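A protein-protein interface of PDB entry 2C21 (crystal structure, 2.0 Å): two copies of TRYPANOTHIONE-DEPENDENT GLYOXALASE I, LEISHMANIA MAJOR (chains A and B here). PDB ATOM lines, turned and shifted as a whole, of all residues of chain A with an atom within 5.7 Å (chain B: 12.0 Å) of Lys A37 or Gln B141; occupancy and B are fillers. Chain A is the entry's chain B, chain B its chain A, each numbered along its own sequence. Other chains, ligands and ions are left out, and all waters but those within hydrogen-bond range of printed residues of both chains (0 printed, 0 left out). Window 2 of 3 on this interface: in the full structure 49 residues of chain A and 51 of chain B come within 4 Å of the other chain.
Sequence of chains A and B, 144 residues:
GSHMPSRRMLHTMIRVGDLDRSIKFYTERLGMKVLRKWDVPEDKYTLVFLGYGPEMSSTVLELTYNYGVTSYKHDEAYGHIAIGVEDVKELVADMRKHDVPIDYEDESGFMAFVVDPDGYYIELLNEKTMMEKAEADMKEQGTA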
ATOM      1  N   ASP A  20      32.890 -16.072  -3.894  1.00  0.00           N
ATOM      2  CA  ASP A  20      32.572 -14.828  -3.177  1.00  0.00           C
ATOM      3  C   ASP A  20      32.156 -13.741  -4.154  1.00  0.00           C
ATOM      4  O   ASP A  20      31.271 -12.942  -3.868  1.00  0.00           O
ATOM      5  CB  ASP A  20      33.749 -14.372  -2.340  1.00  0.00           C
ATOM      6  CG  ASP A  20      33.951 -15.220  -1.076  1.00  0.00           C
ATOM      7  OD1 ASP A  20      33.048 -15.960  -0.643  1.00  0.00           O
ATOM      8  OD2 ASP A  20      35.039 -15.139  -0.519  1.00  0.00           O
ATOM      9  N   ILE A  23      28.548 -14.574  -5.100  1.00  0.00           N
ATOM     10  CA  ILE A  23      27.666 -14.223  -3.988  1.00  0.00           C
ATOM     11  C   ILE A  23      27.448 -12.710  -3.906  1.00  0.00           C
ATOM     12  O   ILE A  23      26.317 -12.244  -3.718  1.00  0.00           O
ATOM     13  CB  ILE A  23      28.191 -14.769  -2.659  1.00  0.00           C
ATOM     14  CG1 ILE A  23      28.080 -16.300  -2.638  1.00  0.00           C
ATOM     15  CG2 ILE A  23      27.455 -14.145  -1.479  1.00  0.00           C
ATOM     16  CD1 ILE A  23      28.873 -16.960  -1.458  1.00  0.00           C
ATOM     17  N   VAL A  34      21.792 -14.962   1.084  1.00  0.00           N
ATOM     18  CA  VAL A  34      22.388 -16.273   1.254  1.00  0.00           C
ATOM     19  C   VAL A  34      21.541 -17.083   2.248  1.00  0.00           C
ATOM     20  O   VAL A  34      21.259 -16.610   3.345  1.00  0.00           O
ATOM     21  CB  VAL A  34      23.831 -16.161   1.782  1.00  0.00           C
ATOM     22  CG1 VAL A  34      24.363 -17.544   2.242  1.00  0.00           C
ATOM     23  CG2 VAL A  34      24.721 -15.555   0.697  1.00  0.00           C
ATOM     24  N   LEU A  35      21.157 -18.296   1.851  1.00  0.00           N
ATOM     25  CA  LEU A  35      20.260 -19.138   2.643  1.00  0.00           C
ATOM     26  C   LEU A  35      21.078 -20.098   3.491  1.00  0.00           C
ATOM     27  O   LEU A  35      20.855 -20.226   4.694  1.00  0.00           O
ATOM     28  CB  LEU A  35      19.266 -19.877   1.726  1.00  0.00           C
ATOM     29  CG  LEU A  35      18.474 -18.959   0.772  1.00  0.00           C
ATOM     30  CD1 LEU A  35      17.604 -19.722  -0.238  1.00  0.00           C
ATOM     31  CD2 LEU A  35      17.610 -17.993   1.543  1.00  0.00           C
ATOM     32  N   ARG A  36      22.059 -20.737   2.860  1.00  0.00           N
ATOM     33  CA  ARG A  36      22.931 -21.661   3.531  1.00  0.00           C
ATOM     34  C   ARG A  36      24.088 -22.028   2.609  1.00  0.00           C
ATOM     35  O   ARG A  36      24.018 -21.841   1.403  1.00  0.00           O
ATOM     36  CB  ARG A  36      22.182 -22.933   3.947  1.00  0.00           C
ATOM     37  CG  ARG A  36      21.418 -23.586   2.824  1.00  0.00           C
ATOM     38  CD  ARG A  36      20.780 -24.890   3.248  1.00  0.00           C
ATOM     39  NE  ARG A  36      20.190 -25.587   2.106  1.00  0.00           N
ATOM     40  CZ  ARG A  36      20.163 -26.910   1.950  1.00  0.00           C
ATOM     41  NH1 ARG A  36      20.709 -27.727   2.852  1.00  0.00           N
ATOM     42  NH2 ARG A  36      19.595 -27.429   0.874  1.00  0.00           N
ATOM     43  N   LYS A  37      25.141 -22.554   3.208  1.00  0.00           N
ATOM     44  CA  LYS A  37      26.250 -23.109   2.478  1.00  0.00           C
ATOM     45  C   LYS A  37      26.462 -24.550   2.878  1.00  0.00           C
ATOM     46  O   LYS A  37      26.103 -24.971   3.997  1.00  0.00           O
ATOM     47  CB  LYS A  37      27.518 -22.318   2.763  1.00  0.00           C
ATOM     48  CG  LYS A  37      27.393 -20.824   2.488  1.00  0.00           C
ATOM     49  CD  LYS A  37      28.750 -20.128   2.647  1.00  0.00           C
ATOM     50  CE  LYS A  37      28.709 -18.659   2.203  1.00  0.00           C
ATOM     51  NZ  LYS A  37      29.975 -17.922   2.555  1.00  0.00           N
ATOM     52  N   TRP A  38      27.077 -25.295   1.967  1.00  0.00           N
ATOM     53  CA  TRP A  38      27.395 -26.687   2.201  1.00  0.00           C
ATOM     54  C   TRP A  38      28.713 -27.031   1.549  1.00  0.00           C
ATOM     55  O   TRP A  38      28.785 -27.250   0.333  1.00  0.00           O
ATOM     56  CB  TRP A  38      26.288 -27.589   1.645  1.00  0.00           C
ATOM     57  CG  TRP A  38      26.376 -28.973   2.197  1.00  0.00           C
ATOM     58  CD1 TRP A  38      26.598 -30.129   1.501  1.00  0.00           C
ATOM     59  CD2 TRP A  38      26.274 -29.347   3.578  1.00  0.00           C
ATOM     60  NE1 TRP A  38      26.614 -31.203   2.363  1.00  0.00           N
ATOM     61  CE2 TRP A  38      26.419 -30.750   3.642  1.00  0.00           C
ATOM     62  CE3 TRP A  38      26.049 -28.629   4.770  1.00  0.00           C
ATOM     63  CZ2 TRP A  38      26.375 -31.446   4.847  1.00  0.00           C
ATOM     64  CZ3 TRP A  38      26.012 -29.319   5.962  1.00  0.00           C
ATOM     65  CH2 TRP A  38      26.164 -30.716   5.995  1.00  0.00           C
ATOM     66  N   ASP A  39      29.765 -27.055   2.361  1.00  0.00           N
ATOM     67  CA  ASP A  39      31.104 -27.384   1.873  1.00  0.00           C
ATOM     68  C   ASP A  39      31.317 -28.903   1.881  1.00  0.00           C
ATOM     69  O   ASP A  39      31.006 -29.581   2.867  1.00  0.00           O
ATOM     70  CB  ASP A  39      32.168 -26.713   2.745  1.00  0.00           C
ATOM     71  CG  ASP A  39      33.541 -26.735   2.110  1.00  0.00           C
ATOM     72  OD1 ASP A  39      33.663 -26.857   0.873  1.00  0.00           O
ATOM     73  OD2 ASP A  39      34.527 -26.636   2.854  1.00  0.00           O
ATOM     74  N   THR A  46      32.096 -26.706  -3.052  1.00  0.00           N
ATOM     75  CA  THR A  46      31.270 -25.957  -2.104  1.00  0.00           C
ATOM     76  C   THR A  46      29.981 -25.549  -2.807  1.00  0.00           C
ATOM     77  O   THR A  46      30.030 -25.093  -3.954  1.00  0.00           O
ATOM     78  CB  THR A  46      31.954 -24.660  -1.627  1.00  0.00           C
ATOM     79  OG1 THR A  46      33.299 -24.934  -1.234  1.00  0.00           O
ATOM     80  CG2 THR A  46      31.205 -24.062  -0.452  1.00  0.00           C
ATOM     81  N   LEU A  47      28.857 -25.739  -2.124  1.00  0.00           N
ATOM     82  CA  LEU A  47      27.545 -25.260  -2.564  1.00  0.00           C
ATOM     83  C   LEU A  47      27.122 -24.068  -1.722  1.00  0.00           C
ATOM     84  O   LEU A  47      27.353 -24.044  -0.494  1.00  0.00           O
ATOM     85  CB  LEU A  47      26.457 -26.343  -2.411  1.00  0.00           C
ATOM     86  CG  LEU A  47      26.750 -27.714  -3.019  1.00  0.00           C
ATOM     87  CD1 LEU A  47      25.633 -28.696  -2.689  1.00  0.00           C
ATOM     88  CD2 LEU A  47      26.968 -27.595  -4.518  1.00  0.00           C
ATOM     89  N   VAL A  48      26.470 -23.104  -2.374  1.00  0.00           N
ATOM     90  CA  VAL A  48      25.747 -22.034  -1.674  1.00  0.00           C
ATOM     91  C   VAL A  48      24.357 -21.865  -2.293  1.00  0.00           C
ATOM     92  O   VAL A  48      24.223 -21.885  -3.513  1.00  0.00           O
ATOM     93  CB  VAL A  48      26.498 -20.698  -1.747  1.00  0.00           C
ATOM     94  CG1 VAL A  48      25.727 -19.585  -1.009  1.00  0.00           C
ATOM     95  CG2 VAL A  48      27.862 -20.851  -1.137  1.00  0.00           C
ATOM     96  N   PHE A  49      23.336 -21.710  -1.446  1.00  0.00           N
ATOM     97  CA  PHE A  49      21.977 -21.436  -1.919  1.00  0.00           C
ATOM     98  C   PHE A  49      21.630 -19.993  -1.644  1.00  0.00           C
ATOM     99  O   PHE A  49      21.886 -19.485  -0.555  1.00  0.00           O
ATOM    100  CB  PHE A  49      20.972 -22.368  -1.234  1.00  0.00           C
ATOM    101  CG  PHE A  49      21.177 -23.811  -1.570  1.00  0.00           C
ATOM    102  CD1 PHE A  49      22.120 -24.571  -0.882  1.00  0.00           C
ATOM    103  CD2 PHE A  49      20.460 -24.407  -2.588  1.00  0.00           C
ATOM    104  CE1 PHE A  49      22.307 -25.921  -1.183  1.00  0.00           C
ATOM    105  CE2 PHE A  49      20.649 -25.755  -2.910  1.00  0.00           C
ATOM    106  CZ  PHE A  49      21.570 -26.516  -2.199  1.00  0.00           C
ATOM    107  N   MET B 130      14.968 -32.977   2.045  1.00  0.00           N
ATOM    108  CA  MET B 130      15.697 -31.781   1.605  1.00  0.00           C
ATOM    109  C   MET B 130      15.365 -30.553   2.461  1.00  0.00           C
ATOM    110  O   MET B 130      16.259 -29.788   2.827  1.00  0.00           O
ATOM    111  CB  MET B 130      15.416 -31.492   0.127  1.00  0.00           C
ATOM    112  CG  MET B 130      16.149 -30.276  -0.435  1.00  0.00           C
ATOM    113  SD  MET B 130      17.935 -30.458  -0.491  1.00  0.00           S
ATOM    114  CE  MET B 130      18.371 -29.159  -1.662  1.00  0.00           C
ATOM    115  N   MET B 131      14.085 -30.371   2.778  1.00  0.00           N
ATOM    116  CA  MET B 131      13.652 -29.188   3.520  1.00  0.00           C
ATOM    117  C   MET B 131      14.008 -29.267   5.015  1.00  0.00           C
ATOM    118  O   MET B 131      14.326 -28.246   5.641  1.00  0.00           O
ATOM    119  CB  MET B 131      12.139 -28.961   3.335  1.00  0.00           C
ATOM    120  CG  MET B 131      11.702 -28.571   1.914  1.00  0.00           C
ATOM    121  SD  MET B 131      12.663 -27.243   1.163  1.00  0.00           S
ATOM    122  CE  MET B 131      13.619 -28.161  -0.025  1.00  0.00           C
ATOM    123  N   GLU B 132      13.948 -30.472   5.580  1.00  0.00           N
ATOM    124  CA  GLU B 132      14.404 -30.687   6.953  1.00  0.00           C
ATOM    125  C   GLU B 132      15.874 -30.277   7.064  1.00  0.00           C
ATOM    126  O   GLU B 132      16.253 -29.534   7.973  1.00  0.00           O
ATOM    127  CB  GLU B 132      14.250 -32.160   7.371  1.00  0.00           C
ATOM    128  CG  GLU B 132      12.822 -32.625   7.578  1.00  0.00           C
ATOM    129  CD  GLU B 132      12.721 -34.098   7.955  1.00  0.00           C
ATOM    130  OE1 GLU B 132      13.762 -34.728   8.261  1.00  0.00           O
ATOM    131  OE2 GLU B 132      11.588 -34.628   7.934  1.00  0.00           O
ATOM    132  N   LYS B 133      16.686 -30.762   6.124  1.00  0.00           N
ATOM    133  CA  LYS B 133      18.122 -30.450   6.082  1.00  0.00           C
ATOM    134  C   LYS B 133      18.356 -28.964   5.868  1.00  0.00           C
ATOM    135  O   LYS B 133      19.144 -28.358   6.567  1.00  0.00           O
ATOM    136  CB  LYS B 133      18.827 -31.260   4.982  1.00  0.00           C
ATOM    137  CG  LYS B 133      20.347 -31.052   4.889  1.00  0.00           C
ATOM    138  CD  LYS B 133      20.997 -31.150   6.267  1.00  0.00           C
ATOM    139  CE  LYS B 133      22.461 -31.585   6.222  1.00  0.00           C
ATOM    140  NZ  LYS B 133      22.882 -32.109   7.557  1.00  0.00           N
ATOM    141  N   ALA B 134      17.681 -28.369   4.886  1.00  0.00           N
ATOM    142  CA  ALA B 134      17.804 -26.935   4.648  1.00  0.00           C
ATOM    143  C   ALA B 134      17.474 -26.126   5.905  1.00  0.00           C
ATOM    144  O   ALA B 134      18.209 -25.219   6.282  1.00  0.00           O
ATOM    145  CB  ALA B 134      16.906 -26.515   3.496  1.00  0.00           C
ATOM    146  N   GLU B 135      16.386 -26.485   6.579  1.00  0.00           N
ATOM    147  CA  GLU B 135      15.996 -25.784   7.796  1.00  0.00           C
ATOM    148  C   GLU B 135      17.067 -25.870   8.881  1.00  0.00           C
ATOM    149  O   GLU B 135      17.438 -24.836   9.478  1.00  0.00           O
ATOM    150  CB  GLU B 135      14.671 -26.319   8.344  1.00  0.00           C
ATOM    151  CG  GLU B 135      14.211 -25.576   9.599  1.00  0.00           C
ATOM    152  CD  GLU B 135      13.094 -26.283  10.332  1.00  0.00           C
ATOM    153  OE1 GLU B 135      12.375 -27.080   9.699  1.00  0.00           O
ATOM    154  OE2 GLU B 135      12.947 -26.033  11.543  1.00  0.00           O
ATOM    155  N   ALA B 136      17.556 -27.083   9.146  1.00  0.00           N
ATOM    156  CA  ALA B 136      18.583 -27.281  10.181  1.00  0.00           C
ATOM    157  C   ALA B 136      19.863 -26.517   9.830  1.00  0.00           C
ATOM    158  O   ALA B 136      20.481 -25.893  10.688  1.00  0.00           O
ATOM    159  CB  ALA B 136      18.880 -28.760  10.363  1.00  0.00           C
ATOM    160  N   ASP B 137      20.252 -26.553   8.560  1.00  0.00           N
ATOM    161  CA  ASP B 137      21.448 -25.829   8.125  1.00  0.00           C
ATOM    162  C   ASP B 137      21.272 -24.316   8.357  1.00  0.00           C
ATOM    163  O   ASP B 137      22.181 -23.646   8.837  1.00  0.00           O
ATOM    164  CB  ASP B 137      21.770 -26.109   6.642  1.00  0.00           C
ATOM    165  CG  ASP B 137      22.368 -27.504   6.395  1.00  0.00           C
ATOM    166  OD1 ASP B 137      22.715 -28.235   7.357  1.00  0.00           O
ATOM    167  OD2 ASP B 137      22.505 -27.872   5.203  1.00  0.00           O
ATOM    168  N   MET B 138      20.108 -23.773   8.005  1.00  0.00           N
ATOM    169  CA  MET B 138      19.850 -22.343   8.179  1.00  0.00           C
ATOM    170  C   MET B 138      19.914 -21.938   9.652  1.00  0.00           C
ATOM    171  O   MET B 138      20.476 -20.900   9.996  1.00  0.00           O
ATOM    172  CB  MET B 138      18.482 -21.972   7.609  1.00  0.00           C
ATOM    173  CG  MET B 138      18.407 -21.994   6.087  1.00  0.00           C
ATOM    174  SD  MET B 138      16.827 -21.403   5.467  1.00  0.00           S
ATOM    175  CE  MET B 138      17.009 -19.636   5.636  1.00  0.00           C
ATOM    176  N   LYS B 139      19.332 -22.754  10.524  1.00  0.00           N
ATOM    177  CA  LYS B 139      19.348 -22.450  11.953  1.00  0.00           C
ATOM    178  C   LYS B 139      20.780 -22.493  12.506  1.00  0.00           C
ATOM    179  O   LYS B 139      21.217 -21.558  13.178  1.00  0.00           O
ATOM    180  CB  LYS B 139      18.396 -23.381  12.715  1.00  0.00           C
ATOM    181  CG  LYS B 139      16.919 -23.044  12.444  1.00  0.00           C
ATOM    182  CD  LYS B 139      15.934 -23.913  13.223  1.00  0.00           C
ATOM    183  CE  LYS B 139      14.513 -23.370  13.090  1.00  0.00           C
ATOM    184  NZ  LYS B 139      13.508 -24.081  13.952  1.00  0.00           N
ATOM    185  N   GLU B 140      21.511 -23.556  12.184  1.00  0.00           N
ATOM    186  CA  GLU B 140      22.926 -23.671  12.557  1.00  0.00           C
ATOM    187  C   GLU B 140      23.774 -22.497  12.033  1.00  0.00           C
ATOM    188  O   GLU B 140      24.621 -21.966  12.751  1.00  0.00           O
ATOM    189  CB  GLU B 140      23.503 -24.998  12.045  1.00  0.00           C
ATOM    190  CG  GLU B 140      24.997 -25.158  12.258  1.00  0.00           C
ATOM    191  CD  GLU B 140      25.447 -26.605  12.200  1.00  0.00           C
ATOM    192  OE1 GLU B 140      25.347 -27.229  11.121  1.00  0.00           O
ATOM    193  OE2 GLU B 140      25.911 -27.116  13.236  1.00  0.00           O
ATOM    194  N   GLN B 141      23.538 -22.089  10.792  1.00  0.00           N
ATOM    195  CA  GLN B 141      24.339 -21.026  10.167  1.00  0.00           C
ATOM    196  C   GLN B 141      23.844 -19.602  10.487  1.00  0.00           C
ATOM    197  O   GLN B 141      24.480 -18.627  10.100  1.00  0.00           O
ATOM    198  CB  GLN B 141      24.460 -21.272   8.653  1.00  0.00           C
ATOM    199  CG  GLN B 141      25.258 -22.548   8.359  1.00  0.00           C
ATOM    200  CD  GLN B 141      25.234 -22.974   6.906  1.00  0.00           C
ATOM    201  OE1 GLN B 141      25.098 -22.145   6.015  1.00  0.00           O
ATOM    202  NE2 GLN B 141      25.393 -24.280   6.661  1.00  0.00           N
ATOM    203  N   GLY B 142      22.748 -19.483  11.233  1.00  0.00           N
ATOM    204  CA  GLY B 142      22.243 -18.177  11.676  1.00  0.00           C
ATOM    205  C   GLY B 142      21.566 -17.330  10.604  1.00  0.00           C
ATOM    206  O   GLY B 142      21.535 -16.101  10.700  1.00  0.00           O
ATOM    207  N   THR B 143      21.021 -17.979   9.579  1.00  0.00           N
ATOM    208  CA  THR B 143      20.339 -17.269   8.496  1.00  0.00           C
ATOM    209  C   THR B 143      18.827 -17.362   8.638  1.00  0.00           C
ATOM    210  O   THR B 143      18.112 -16.462   8.196  1.00  0.00           O
ATOM    211  CB  THR B 143      20.736 -17.814   7.135  1.00  0.00           C
ATOM    212  OG1 THR B 143      20.328 -19.181   7.030  1.00  0.00           O
ATOM    213  CG2 THR B 143      22.242 -17.711   6.945  1.00  0.00           C
ATOM    214  N   ALA B 144      18.346 -18.455   9.232  1.00  0.00           N
ATOM    215  CA  ALA B 144      16.958 -18.550   9.671  1.00  0.00           C
ATOM    216  C   ALA B 144      16.711 -17.537  10.784  1.00  0.00           C
ATOM    217  O   ALA B 144      16.852 -17.849  11.967  1.00  0.00           O
ATOM    218  CB  ALA B 144      16.638 -19.968  10.159  1.00  0.00           C
ATOM    219  OXT ALA B 144      16.379 -16.381  10.521  1.00  0.00           O
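SD of Met B130 sits close to NH2 of Arg A36, at 3.7 Å. OD2 of Asp B137 lies within salt-bridge range of NH1 of Arg A36 (3.0 Å). The side-chain amide oxygen (OE1) of Gln B141 lies within hydrogen-bond range of the backbone NH (N) of Lys A37 (2.8 Å). O of Leu A35 sits at hydrogen-bond distance from OG1 of Thr B143.
The backbone NH of Phe A49 is in hydrogen-bond range of the backbone carbonyl oxygen of Arg A36 (2.9 Å). N of Thr B143 lies within hydrogen-bond range of O of Met B138, 3.0 Å away. N of Leu A35 sits at hydrogen-bond distance from O of Phe A49 (2.8 Å). The backbone carbonyl oxygen (O) of Met B138 sits at hydrogen-bond distance from the backbone NH (N) of Ala B144, 3.3 Å away. The backbone carbonyl oxygen of Leu A47 sits at hydrogen-bond distance from the backbone NH of Trp A38 (2.8 Å). OD1 of Asp B137 lies within salt-bridge range of NZ of Lys B133 (3.9 Å).
Among the printed residues, pairs that only touch across the chains: Leu A35 with Met B138 (3.3 Å), Arg A36 with Gln B141 (3.3 Å), Arg A36 with Ala B134 (3.5 Å), Trp A38 with Asp B137 (3.6 Å), Trp A38 with Lys B133 (3.8 Å), Val A34 with Thr B143 (3.9 Å) and Arg A36 with Lys B133 (3.9 Å).
Lys A37 touches one residue of chain B. Gln B141 touches just these residues of chain A: Arg A36 and Lys A37. Printed residues of chain B within 4 Å of Val A34: Thr B143. Arg A36 touches five residues of chain B. Of the printed residues of chain A, Thr B143 touches Val A34 (3.9 Å) and Leu A35 (2.6 Å). Printed residues of chain A within 4 Å of Lys B133: Arg A36 (3.9 Å) and Trp A38 (3.8 Å). Of the printed residues of chain A, Asp B137 touches Arg A36 (3.0 Å) and Trp A38 (3.6 Å). Met B131 touches none of the printed residues of chain A. Lys B139 touches none of the printed residues of chain A.
Printed residues of chain B that touch a printed residue of chain A: Met B130, Lys B133, Ala B134, Asp B137, Met B138, Gln B141 and Thr B143. Hydrophobic or aromatic side chains of chain B that line the printed part of chain A: Met B130, Ala B134 and Met B138. Of the 12 printed residues of chain A, 5 touch a printed residue of chain B. Hydrophobic or aromatic side chains of chain A within 4 Å of the printed part of chain B: Trp A38. Among the printed residues, Asp or Glu carboxylates within 4 Å of a Lys or Arg side-chain nitrogen of the other chain: Arg A36 with Asp B137 (3.0 Å).
No position is printed for both chains.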
